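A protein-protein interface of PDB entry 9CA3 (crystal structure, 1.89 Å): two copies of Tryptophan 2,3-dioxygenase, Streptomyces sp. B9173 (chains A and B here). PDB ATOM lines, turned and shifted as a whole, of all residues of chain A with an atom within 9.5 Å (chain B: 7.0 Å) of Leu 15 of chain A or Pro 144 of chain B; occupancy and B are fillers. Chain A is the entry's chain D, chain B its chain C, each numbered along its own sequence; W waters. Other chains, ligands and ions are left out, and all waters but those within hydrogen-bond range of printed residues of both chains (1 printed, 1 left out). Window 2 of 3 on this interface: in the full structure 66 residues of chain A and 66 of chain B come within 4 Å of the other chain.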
ATOM      1  N   SER A   6       7.818 -14.538 -13.463  1.00  0.00           N
ATOM      2  CA  SER A   6       6.636 -14.985 -12.739  1.00  0.00           C
ATOM      3  C   SER A   6       7.071 -15.672 -11.457  1.00  0.00           C
ATOM      4  O   SER A   6       8.032 -16.445 -11.454  1.00  0.00           O
ATOM      5  CB  SER A   6       5.783 -15.952 -13.569  1.00  0.00           C
ATOM      6  OG  SER A   6       4.711 -16.447 -12.794  1.00  0.00           O
ATOM      7  N   ASN A   8       5.092 -17.771 -10.041  1.00  0.00           N
ATOM      8  CA  ASN A   8       4.459 -19.086 -10.145  1.00  0.00           C
ATOM      9  C   ASN A   8       4.393 -19.445 -11.622  1.00  0.00           C
ATOM     10  O   ASN A   8       3.323 -19.443 -12.237  1.00  0.00           O
ATOM     11  CB  ASN A   8       3.084 -19.090  -9.470  1.00  0.00           C
ATOM     12  CG  ASN A   8       2.146 -18.009 -10.006  1.00  0.00           C
ATOM     13  OD1 ASN A   8       2.574 -16.911 -10.400  1.00  0.00           O
ATOM     14  ND2 ASN A   8       0.865 -18.314 -10.017  1.00  0.00           N
ATOM     15  N   GLU A  11       2.018 -22.268 -13.411  1.00  0.00           N
ATOM     16  CA  GLU A  11       0.581 -22.048 -13.290  1.00  0.00           C
ATOM     17  C   GLU A  11      -0.114 -22.250 -14.625  1.00  0.00           C
ATOM     18  O   GLU A  11       0.259 -21.607 -15.614  1.00  0.00           O
ATOM     19  CB  GLU A  11       0.286 -20.634 -12.783  1.00  0.00           C
ATOM     20  CG  GLU A  11      -1.165 -20.441 -12.428  1.00  0.00           C
ATOM     21  CD  GLU A  11      -1.486 -21.126 -11.131  1.00  0.00           C
ATOM     22  OE1 GLU A  11      -0.604 -21.116 -10.234  1.00  0.00           O
ATOM     23  OE2 GLU A  11      -2.567 -21.734 -11.026  1.00  0.00           O
ATOM     24  N   PRO A  12      -1.094 -23.155 -14.709  1.00  0.00           N
ATOM     25  CA  PRO A  12      -1.877 -23.263 -15.945  1.00  0.00           C
ATOM     26  C   PRO A  12      -2.488 -21.929 -16.318  1.00  0.00           C
ATOM     27  O   PRO A  12      -2.001 -21.251 -17.230  1.00  0.00           O
ATOM     28  CB  PRO A  12      -2.948 -24.310 -15.603  1.00  0.00           C
ATOM     29  CG  PRO A  12      -2.941 -24.422 -14.099  1.00  0.00           C
ATOM     30  CD  PRO A  12      -1.520 -24.148 -13.703  1.00  0.00           C
ATOM     31  N   ASN A  13      -3.528 -21.535 -15.579  1.00  0.00           N
ATOM     32  CA  ASN A  13      -4.292 -20.321 -15.849  1.00  0.00           C
ATOM     33  C   ASN A  13      -3.400 -19.082 -15.835  1.00  0.00           C
ATOM     34  O   ASN A  13      -2.920 -18.666 -14.775  1.00  0.00           O
ATOM     35  CB  ASN A  13      -5.428 -20.201 -14.826  1.00  0.00           C
ATOM     36  CG  ASN A  13      -6.460 -19.161 -15.214  1.00  0.00           C
ATOM     37  OD1 ASN A  13      -6.222 -18.326 -16.089  1.00  0.00           O
ATOM     38  ND2 ASN A  13      -7.627 -19.213 -14.563  1.00  0.00           N
ATOM     39  N   ALA A  14      -3.181 -18.480 -17.008  1.00  0.00           N
ATOM     40  CA  ALA A  14      -2.300 -17.319 -17.101  1.00  0.00           C
ATOM     41  C   ALA A  14      -2.798 -16.143 -16.274  1.00  0.00           C
ATOM     42  O   ALA A  14      -1.990 -15.294 -15.881  1.00  0.00           O
ATOM     43  CB  ALA A  14      -2.141 -16.885 -18.559  1.00  0.00           C
ATOM     44  N   LEU A  15      -4.104 -16.078 -15.993  1.00  0.00           N
ATOM     45  CA  LEU A  15      -4.669 -15.018 -15.167  1.00  0.00           C
ATOM     46  C   LEU A  15      -4.308 -15.150 -13.695  1.00  0.00           C
ATOM     47  O   LEU A  15      -4.493 -14.188 -12.939  1.00  0.00           O
ATOM     48  CB  LEU A  15      -6.199 -14.972 -15.322  1.00  0.00           C
ATOM     49  CG  LEU A  15      -6.790 -14.633 -16.701  1.00  0.00           C
ATOM     50  CD1 LEU A  15      -8.328 -14.607 -16.650  1.00  0.00           C
ATOM     51  CD2 LEU A  15      -6.253 -13.301 -17.209  1.00  0.00           C
ATOM     52  N   LEU A  16      -3.788 -16.290 -13.272  1.00  0.00           N
ATOM     53  CA  LEU A  16      -3.354 -16.493 -11.902  1.00  0.00           C
ATOM     54  C   LEU A  16      -1.860 -16.270 -11.737  1.00  0.00           C
ATOM     55  O   LEU A  16      -1.337 -16.464 -10.641  1.00  0.00           O
ATOM     56  CB  LEU A  16      -3.718 -17.914 -11.426  1.00  0.00           C
ATOM     57  CG  LEU A  16      -5.199 -18.313 -11.344  1.00  0.00           C
ATOM     58  CD1 LEU A  16      -5.438 -19.371 -10.253  1.00  0.00           C
ATOM     59  CD2 LEU A  16      -6.055 -17.100 -11.083  1.00  0.00           C
ATOM     60  N   SER A  17      -1.167 -15.894 -12.803  1.00  0.00           N
ATOM     61  CA  SER A  17       0.274 -15.719 -12.764  1.00  0.00           C
ATOM     62  C   SER A  17       0.621 -14.374 -12.134  1.00  0.00           C
ATOM     63  O   SER A  17       0.072 -13.342 -12.527  1.00  0.00           O
ATOM     64  CB  SER A  17       0.850 -15.787 -14.175  1.00  0.00           C
ATOM     65  OG  SER A  17       2.245 -15.525 -14.155  1.00  0.00           O
ATOM     66  N   TYR A  18       1.526 -14.385 -11.165  1.00  0.00           N
ATOM     67  CA  TYR A  18       2.078 -13.133 -10.632  1.00  0.00           C
ATOM     68  C   TYR A  18       3.269 -12.724 -11.485  1.00  0.00           C
ATOM     69  O   TYR A  18       4.400 -13.147 -11.248  1.00  0.00           O
ATOM     70  CB  TYR A  18       2.480 -13.286  -9.178  1.00  0.00           C
ATOM     71  CG  TYR A  18       2.569 -11.951  -8.439  1.00  0.00           C
ATOM     72  CD1 TYR A  18       3.729 -11.212  -8.408  1.00  0.00           C
ATOM     73  CD2 TYR A  18       1.464 -11.463  -7.765  1.00  0.00           C
ATOM     74  CE1 TYR A  18       3.772  -9.989  -7.714  1.00  0.00           C
ATOM     75  CE2 TYR A  18       1.492 -10.306  -7.087  1.00  0.00           C
ATOM     76  CZ  TYR A  18       2.614  -9.559  -7.055  1.00  0.00           C
ATOM     77  OH  TYR A  18       2.563  -8.389  -6.341  1.00  0.00           O
ATOM     78  N   ASP A  19       3.016 -11.855 -12.463  1.00  0.00           N
ATOM     79  CA  ASP A  19       4.056 -11.341 -13.343  1.00  0.00           C
ATOM     80  C   ASP A  19       4.749 -10.124 -12.735  1.00  0.00           C
ATOM     81  O   ASP A  19       4.105  -9.216 -12.195  1.00  0.00           O
ATOM     82  CB  ASP A  19       3.451 -10.991 -14.704  1.00  0.00           C
ATOM     83  CG  ASP A  19       2.847 -12.229 -15.398  1.00  0.00           C
ATOM     84  OD1 ASP A  19       3.193 -13.368 -14.988  1.00  0.00           O
ATOM     85  OD2 ASP A  19       2.012 -12.071 -16.315  1.00  0.00           O
ATOM     86  N   HIS B  68      -2.250 -11.613  -3.246  1.00  0.00           N
ATOM     87  CA  HIS B  68      -2.432 -12.392  -4.469  1.00  0.00           C
ATOM     88  C   HIS B  68      -2.327 -13.888  -4.182  1.00  0.00           C
ATOM     89  O   HIS B  68      -3.156 -14.687  -4.626  1.00  0.00           O
ATOM     90  CB  HIS B  68      -1.367 -11.966  -5.481  1.00  0.00           C
ATOM     91  CG  HIS B  68      -1.565 -12.519  -6.854  1.00  0.00           C
ATOM     92  ND1 HIS B  68      -1.091 -13.758  -7.242  1.00  0.00           N
ATOM     93  CD2 HIS B  68      -2.181 -11.990  -7.941  1.00  0.00           C
ATOM     94  CE1 HIS B  68      -1.419 -13.971  -8.506  1.00  0.00           C
ATOM     95  NE2 HIS B  68      -2.059 -12.902  -8.961  1.00  0.00           N
ATOM     96  N   ARG B  72      -5.397 -16.679  -4.757  1.00  0.00           N
ATOM     97  CA  ARG B  72      -5.258 -17.958  -5.469  1.00  0.00           C
ATOM     98  C   ARG B  72      -5.721 -19.139  -4.616  1.00  0.00           C
ATOM     99  O   ARG B  72      -6.414 -20.039  -5.108  1.00  0.00           O
ATOM    100  CB  ARG B  72      -3.805 -18.163  -5.895  1.00  0.00           C
ATOM    101  CG  ARG B  72      -3.426 -17.292  -7.080  1.00  0.00           C
ATOM    102  CD  ARG B  72      -1.932 -17.282  -7.261  1.00  0.00           C
ATOM    103  NE  ARG B  72      -1.397 -18.634  -7.365  1.00  0.00           N
ATOM    104  CZ  ARG B  72      -0.179 -18.992  -6.981  1.00  0.00           C
ATOM    105  NH1 ARG B  72       0.666 -18.117  -6.448  1.00  0.00           N
ATOM    106  NH2 ARG B  72       0.201 -20.259  -7.135  1.00  0.00           N
ATOM    107  N   ILE B  75      -9.442 -19.157  -4.561  1.00  0.00           N
ATOM    108  CA  ILE B  75      -9.993 -19.755  -5.774  1.00  0.00           C
ATOM    109  C   ILE B  75     -10.005 -21.276  -5.653  1.00  0.00           C
ATOM    110  O   ILE B  75     -11.016 -21.929  -5.932  1.00  0.00           O
ATOM    111  CB  ILE B  75      -9.208 -19.293  -7.018  1.00  0.00           C
ATOM    112  CG1 ILE B  75      -9.432 -17.801  -7.274  1.00  0.00           C
ATOM    113  CG2 ILE B  75      -9.628 -20.134  -8.254  1.00  0.00           C
ATOM    114  CD1 ILE B  75      -8.528 -17.205  -8.384  1.00  0.00           C
ATOM    115  N   LEU B  78     -12.773 -22.400  -3.258  1.00  0.00           N
ATOM    116  CA  LEU B  78     -14.122 -22.179  -3.760  1.00  0.00           C
ATOM    117  C   LEU B  78     -14.479 -23.178  -4.850  1.00  0.00           C
ATOM    118  O   LEU B  78     -15.621 -23.654  -4.914  1.00  0.00           O
ATOM    119  CB  LEU B  78     -14.240 -20.740  -4.274  1.00  0.00           C
ATOM    120  CG  LEU B  78     -14.407 -19.710  -3.154  1.00  0.00           C
ATOM    121  CD1 LEU B  78     -14.343 -18.292  -3.737  1.00  0.00           C
ATOM    122  CD2 LEU B  78     -15.708 -19.893  -2.401  1.00  0.00           C
ATOM    123  N   ASP B  79     -13.521 -23.501  -5.719  1.00  0.00           N
ATOM    124  CA  ASP B  79     -13.757 -24.468  -6.786  1.00  0.00           C
ATOM    125  C   ASP B  79     -14.054 -25.855  -6.243  1.00  0.00           C
ATOM    126  O   ASP B  79     -14.658 -26.673  -6.950  1.00  0.00           O
ATOM    127  CB  ASP B  79     -12.551 -24.517  -7.731  1.00  0.00           C
ATOM    128  CG  ASP B  79     -12.528 -23.363  -8.709  1.00  0.00           C
ATOM    129  OD1 ASP B  79     -13.518 -22.601  -8.754  1.00  0.00           O
ATOM    130  OD2 ASP B  79     -11.517 -23.210  -9.437  1.00  0.00           O
ATOM    131  N   ASN B 137      -1.343  -7.321 -10.859  1.00  0.00           N
ATOM    132  CA  ASN B 137      -1.743  -8.706 -10.636  1.00  0.00           C
ATOM    133  C   ASN B 137      -3.004  -8.821  -9.790  1.00  0.00           C
ATOM    134  O   ASN B 137      -3.750  -9.784  -9.945  1.00  0.00           O
ATOM    135  CB  ASN B 137      -0.590  -9.483  -9.992  1.00  0.00           C
ATOM    136  CG  ASN B 137       0.609  -9.583 -10.919  1.00  0.00           C
ATOM    137  OD1 ASN B 137       0.452  -9.949 -12.090  1.00  0.00           O
ATOM    138  ND2 ASN B 137       1.808  -9.245 -10.419  1.00  0.00           N
ATOM    139  N   ARG B 139      -5.554  -6.704  -9.904  1.00  0.00           N
ATOM    140  CA  ARG B 139      -6.616  -6.422 -10.872  1.00  0.00           C
ATOM    141  C   ARG B 139      -6.863  -7.635 -11.768  1.00  0.00           C
ATOM    142  O   ARG B 139      -8.009  -8.024 -12.027  1.00  0.00           O
ATOM    143  CB  ARG B 139      -6.202  -5.208 -11.706  1.00  0.00           C
ATOM    144  CG  ARG B 139      -7.231  -4.684 -12.660  1.00  0.00           C
ATOM    145  CD  ARG B 139      -6.533  -3.881 -13.725  1.00  0.00           C
ATOM    146  NE  ARG B 139      -7.284  -2.708 -14.127  1.00  0.00           N
ATOM    147  CZ  ARG B 139      -7.882  -2.592 -15.303  1.00  0.00           C
ATOM    148  NH1 ARG B 139      -7.942  -3.611 -16.150  1.00  0.00           N
ATOM    149  NH2 ARG B 139      -8.444  -1.432 -15.635  1.00  0.00           N
ATOM    150  N   ARG B 140      -5.783  -8.271 -12.207  1.00  0.00           N
ATOM    151  CA  ARG B 140      -5.893  -9.414 -13.101  1.00  0.00           C
ATOM    152  C   ARG B 140      -6.573 -10.599 -12.403  1.00  0.00           C
ATOM    153  O   ARG B 140      -7.448 -11.246 -12.980  1.00  0.00           O
ATOM    154  CB  ARG B 140      -4.485  -9.751 -13.598  1.00  0.00           C
ATOM    155  CG  ARG B 140      -4.252 -11.073 -14.260  1.00  0.00           C
ATOM    156  CD  ARG B 140      -2.795 -11.498 -14.010  1.00  0.00           C
ATOM    157  NE  ARG B 140      -1.772 -10.877 -14.846  1.00  0.00           N
ATOM    158  CZ  ARG B 140      -1.726 -10.953 -16.167  1.00  0.00           C
ATOM    159  NH1 ARG B 140      -2.648 -11.601 -16.853  1.00  0.00           N
ATOM    160  NH2 ARG B 140      -0.730 -10.359 -16.816  1.00  0.00           N
ATOM    161  N   VAL B 141      -6.205 -10.875 -11.147  1.00  0.00           N
ATOM    162  CA  VAL B 141      -6.706 -12.048 -10.442  1.00  0.00           C
ATOM    163  C   VAL B 141      -8.116 -11.852  -9.913  1.00  0.00           C
ATOM    164  O   VAL B 141      -8.789 -12.838  -9.582  1.00  0.00           O
ATOM    165  CB  VAL B 141      -5.769 -12.435  -9.274  1.00  0.00           C
ATOM    166  CG1 VAL B 141      -6.104 -11.653  -8.001  1.00  0.00           C
ATOM    167  CG2 VAL B 141      -5.853 -13.943  -8.969  1.00  0.00           C
ATOM    168  N   ALA B 142      -8.586 -10.611  -9.823  1.00  0.00           N
ATOM    169  CA  ALA B 142      -9.889 -10.352  -9.232  1.00  0.00           C
ATOM    170  C   ALA B 142     -11.007 -10.985 -10.045  1.00  0.00           C
ATOM    171  O   ALA B 142     -12.023 -11.384  -9.480  1.00  0.00           O
ATOM    172  CB  ALA B 142     -10.112  -8.844  -9.115  1.00  0.00           C
ATOM    173  N   ARG B 143     -10.838 -11.069 -11.365  1.00  0.00           N
ATOM    174  CA  ARG B 143     -11.866 -11.683 -12.202  1.00  0.00           C
ATOM    175  C   ARG B 143     -11.976 -13.179 -11.933  1.00  0.00           C
ATOM    176  O   ARG B 143     -13.091 -13.652 -11.648  1.00  0.00           O
ATOM    177  CB  ARG B 143     -11.591 -11.365 -13.676  1.00  0.00           C
ATOM    178  CG  ARG B 143     -12.021  -9.981 -14.099  1.00  0.00           C
ATOM    179  CD  ARG B 143     -13.523  -9.858 -14.045  1.00  0.00           C
ATOM    180  NE  ARG B 143     -14.039  -9.304 -12.797  1.00  0.00           N
ATOM    181  CZ  ARG B 143     -15.261  -9.561 -12.347  1.00  0.00           C
ATOM    182  NH1 ARG B 143     -16.079 -10.366 -13.006  1.00  0.00           N
ATOM    183  NH2 ARG B 143     -15.665  -9.021 -11.200  1.00  0.00           N
ATOM    184  N   PRO B 144     -10.901 -13.969 -11.985  1.00  0.00           N
ATOM    185  CA  PRO B 144     -11.043 -15.384 -11.602  1.00  0.00           C
ATOM    186  C   PRO B 144     -11.561 -15.570 -10.181  1.00  0.00           C
ATOM    187  O   PRO B 144     -12.266 -16.553  -9.916  1.00  0.00           O
ATOM    188  CB  PRO B 144      -9.619 -15.939 -11.751  1.00  0.00           C
ATOM    189  CG  PRO B 144      -8.909 -14.991 -12.680  1.00  0.00           C
ATOM    190  CD  PRO B 144      -9.559 -13.651 -12.525  1.00  0.00           C
ATOM    191  N   VAL B 145     -11.240 -14.659  -9.255  1.00  0.00           N
ATOM    192  CA  VAL B 145     -11.719 -14.808  -7.881  1.00  0.00           C
ATOM    193  C   VAL B 145     -13.235 -14.686  -7.838  1.00  0.00           C
ATOM    194  O   VAL B 145     -13.935 -15.492  -7.205  1.00  0.00           O
ATOM    195  CB  VAL B 145     -11.061 -13.769  -6.960  1.00  0.00           C
ATOM    196  CG1 VAL B 145     -11.784 -13.725  -5.623  1.00  0.00           C
ATOM    197  CG2 VAL B 145      -9.564 -14.060  -6.806  1.00  0.00           C
ATOM    198  N   TRP B 146     -13.761 -13.666  -8.509  1.00  0.00           N
ATOM    199  CA  TRP B 146     -15.204 -13.471  -8.526  1.00  0.00           C
ATOM    200  C   TRP B 146     -15.904 -14.626  -9.229  1.00  0.00           C
ATOM    201  O   TRP B 146     -16.959 -15.092  -8.783  1.00  0.00           O
ATOM    202  CB  TRP B 146     -15.573 -12.160  -9.226  1.00  0.00           C
ATOM    203  CG  TRP B 146     -17.060 -12.187  -9.359  1.00  0.00           C
ATOM    204  CD1 TRP B 146     -17.796 -12.450 -10.479  1.00  0.00           C
ATOM    205  CD2 TRP B 146     -17.983 -12.030  -8.289  1.00  0.00           C
ATOM    206  NE1 TRP B 146     -19.136 -12.448 -10.167  1.00  0.00           N
ATOM    207  CE2 TRP B 146     -19.276 -12.197  -8.823  1.00  0.00           C
ATOM    208  CE3 TRP B 146     -17.838 -11.760  -6.919  1.00  0.00           C
ATOM    209  CZ2 TRP B 146     -20.426 -12.101  -8.035  1.00  0.00           C
ATOM    210  CZ3 TRP B 146     -18.976 -11.667  -6.136  1.00  0.00           C
ATOM    211  CH2 TRP B 146     -20.257 -11.827  -6.700  1.00  0.00           C
ATOM    212  N   LYS B 147     -15.342 -15.088 -10.342  1.00  0.00           N
ATOM    213  CA  LYS B 147     -15.954 -16.197 -11.055  1.00  0.00           C
ATOM    214  C   LYS B 147     -16.036 -17.433 -10.164  1.00  0.00           C
ATOM    215  O   LYS B 147     -17.070 -18.107 -10.118  1.00  0.00           O
ATOM    216  CB  LYS B 147     -15.177 -16.466 -12.345  1.00  0.00           C
ATOM    217  CG  LYS B 147     -15.523 -15.445 -13.439  1.00  0.00           C
ATOM    218  CD  LYS B 147     -14.878 -15.727 -14.807  1.00  0.00           C
ATOM    219  CE  LYS B 147     -14.693 -14.426 -15.608  1.00  0.00           C
ATOM    220  NZ  LYS B 147     -13.782 -14.610 -16.774  1.00  0.00           N
ATOM    221  N   ALA B 148     -14.990 -17.687  -9.372  1.00  0.00           N
ATOM    222  CA  ALA B 148     -15.021 -18.841  -8.477  1.00  0.00           C
ATOM    223  C   ALA B 148     -16.138 -18.724  -7.448  1.00  0.00           C
ATOM    224  O   ALA B 148     -16.816 -19.717  -7.146  1.00  0.00           O
ATOM    225  CB  ALA B 148     -13.671 -19.001  -7.785  1.00  0.00           C
ATOM    226  N   TYR B 149     -16.351 -17.531  -6.888  1.00  0.00           N
ATOM    227  CA  TYR B 149     -17.442 -17.360  -5.929  1.00  0.00           C
ATOM    228  C   TYR B 149     -18.799 -17.539  -6.610  1.00  0.00           C
ATOM    229  O   TYR B 149     -19.685 -18.248  -6.107  1.00  0.00           O
ATOM    230  CB  TYR B 149     -17.361 -15.980  -5.266  1.00  0.00           C
ATOM    231  CG  TYR B 149     -18.454 -15.817  -4.231  1.00  0.00           C
ATOM    232  CD1 TYR B 149     -18.464 -16.602  -3.088  1.00  0.00           C
ATOM    233  CD2 TYR B 149     -19.480 -14.899  -4.403  1.00  0.00           C
ATOM    234  CE1 TYR B 149     -19.474 -16.497  -2.136  1.00  0.00           C
ATOM    235  CE2 TYR B 149     -20.515 -14.793  -3.455  1.00  0.00           C
ATOM    236  CZ  TYR B 149     -20.498 -15.600  -2.325  1.00  0.00           C
ATOM    237  OH  TYR B 149     -21.504 -15.516  -1.378  1.00  0.00           O
ATOM    238  N   PHE B 251     -14.659  -6.471  -7.172  1.00  0.00           N
ATOM    239  CA  PHE B 251     -15.823  -7.312  -7.413  1.00  0.00           C
ATOM    240  C   PHE B 251     -17.063  -6.451  -7.648  1.00  0.00           C
ATOM    241  O   PHE B 251     -17.986  -6.434  -6.818  1.00  0.00           O
ATOM    242  CB  PHE B 251     -16.066  -8.265  -6.241  1.00  0.00           C
ATOM    243  CG  PHE B 251     -14.799  -8.881  -5.651  1.00  0.00           C
ATOM    244  CD1 PHE B 251     -13.925  -9.623  -6.442  1.00  0.00           C
ATOM    245  CD2 PHE B 251     -14.511  -8.733  -4.297  1.00  0.00           C
ATOM    246  CE1 PHE B 251     -12.782 -10.203  -5.893  1.00  0.00           C
ATOM    247  CE2 PHE B 251     -13.369  -9.311  -3.727  1.00  0.00           C
ATOM    248  CZ  PHE B 251     -12.496 -10.040  -4.528  1.00  0.00           C
HETATM  249  O   HOH W   1      -3.091 -20.684  -8.204  1.00  0.00           O
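The side-chain hydroxyl (OG) of Ser 6 of chain A is in hydrogen-bond range of the side-chain hydroxyl (OG) of Ser 17 of chain A (3.0 Å).
The side-chain amide nitrogen of Asn 8 of chain A is in hydrogen-bond range of the side-chain carboxylate of Glu 11 of chain A (3.2 Å).
ND2 of Asn 8 of chain A sits at hydrogen-bond distance from O of Leu 16 of chain A (2.9 Å).
The side-chain amide oxygen (OD1) of Asn 8 of chain A lies within hydrogen-bond range of the backbone NH (N) of Tyr 18 of chain A.
The backbone NH (N) of Leu 15 of chain A lies close to the side-chain amide oxygen (OD1) of Asn 13 of chain A, at 3.1 Å.
The side-chain carboxylate (OD1) of Asp 19 of chain A is in hydrogen-bond range of the side-chain hydroxyl (OG) of Ser 17 of chain A (2.5 Å).
Water W1 bridges NE of Arg 72 of chain B (2.8 Å) and OE2 of Glu 11 of chain A (3.1 Å).
No position is printed for both chains.
The guanidinium group (NH2) of Arg 72 of chain B lies within salt-bridge range of the side-chain carboxylate (OE1) of Glu 11 of chain A.
OD1 of Asn 137 of chain B sits close to O of Ser 17 of chain A, 3.4 Å away.
ND2 of Asn 137 of chain B is in hydrogen-bond range of O of Asp 19 of chain A, 2.9 Å away.
The side-chain carboxylate (OD2) of Asp 19 of chain A lies within salt-bridge range of the guanidinium group (NH2) of Arg 140 of chain B (3.3 Å).
Arg 72 of chain B touches Asn 8 of chain A.
Ala 14 of chain A touches Arg 140 of chain B (O to NH1, 3.9 Å).
Arg 140 of chain B touches Leu 15 of chain A.
Val 141 of chain B touches Leu 15 of chain A.
Leu 15 of chain A touches Pro 144 of chain B.
Leu 16 of chain A touches His 68 of chain B.
Leu 16 of chain A touches Arg 72 of chain B.
CD2 of Leu 16 of chain A touches CD1 of Ile 75 of chain B, at 3.7 Å.
CD of Arg 140 of chain B touches O of Ser 17 of chain A, 3.7 Å away.
Tyr 18 of chain A touches His 68 of chain B.
Of chain B, only Arg 140 (3.4 Å), Val 141 (3.96 Å) and Pro 144 (3.8 Å) come within 4 Å of Leu 15 of chain A.
Printed residues of chain B within 4 Å of Ser 17 of chain A: Asn 137 (3.4 Å) and Arg 140 (3.7 Å).
Printed residues of chain B within 4 Å of Tyr 18 of chain A: His 68 and Asn 137.
Printed residues of chain A within 4 Å of Arg 72 of chain B: Asn 8, Glu 11 and Leu 16.
Of the printed residues of chain A, Arg 140 of chain B touches Ala 14 (3.9 Å), Leu 15 (3.4 Å), Ser 17 (3.7 Å) and Asp 19 (3.3 Å).
Pro 144 of chain B touches just these residues of chain A: Leu 15 (3.8 Å) and Leu 16 (3.8 Å).
No residue of chain A comes within 4 Å of Val 145 of chain B.
The nearest residue of chain B that does not touch Leu 15 of chain A is His 68 of chain B (4.8 Å).
The nearest printed residue of chain B that does not touch Asp 19 of chain A is His 68 of chain B (6.3 Å).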
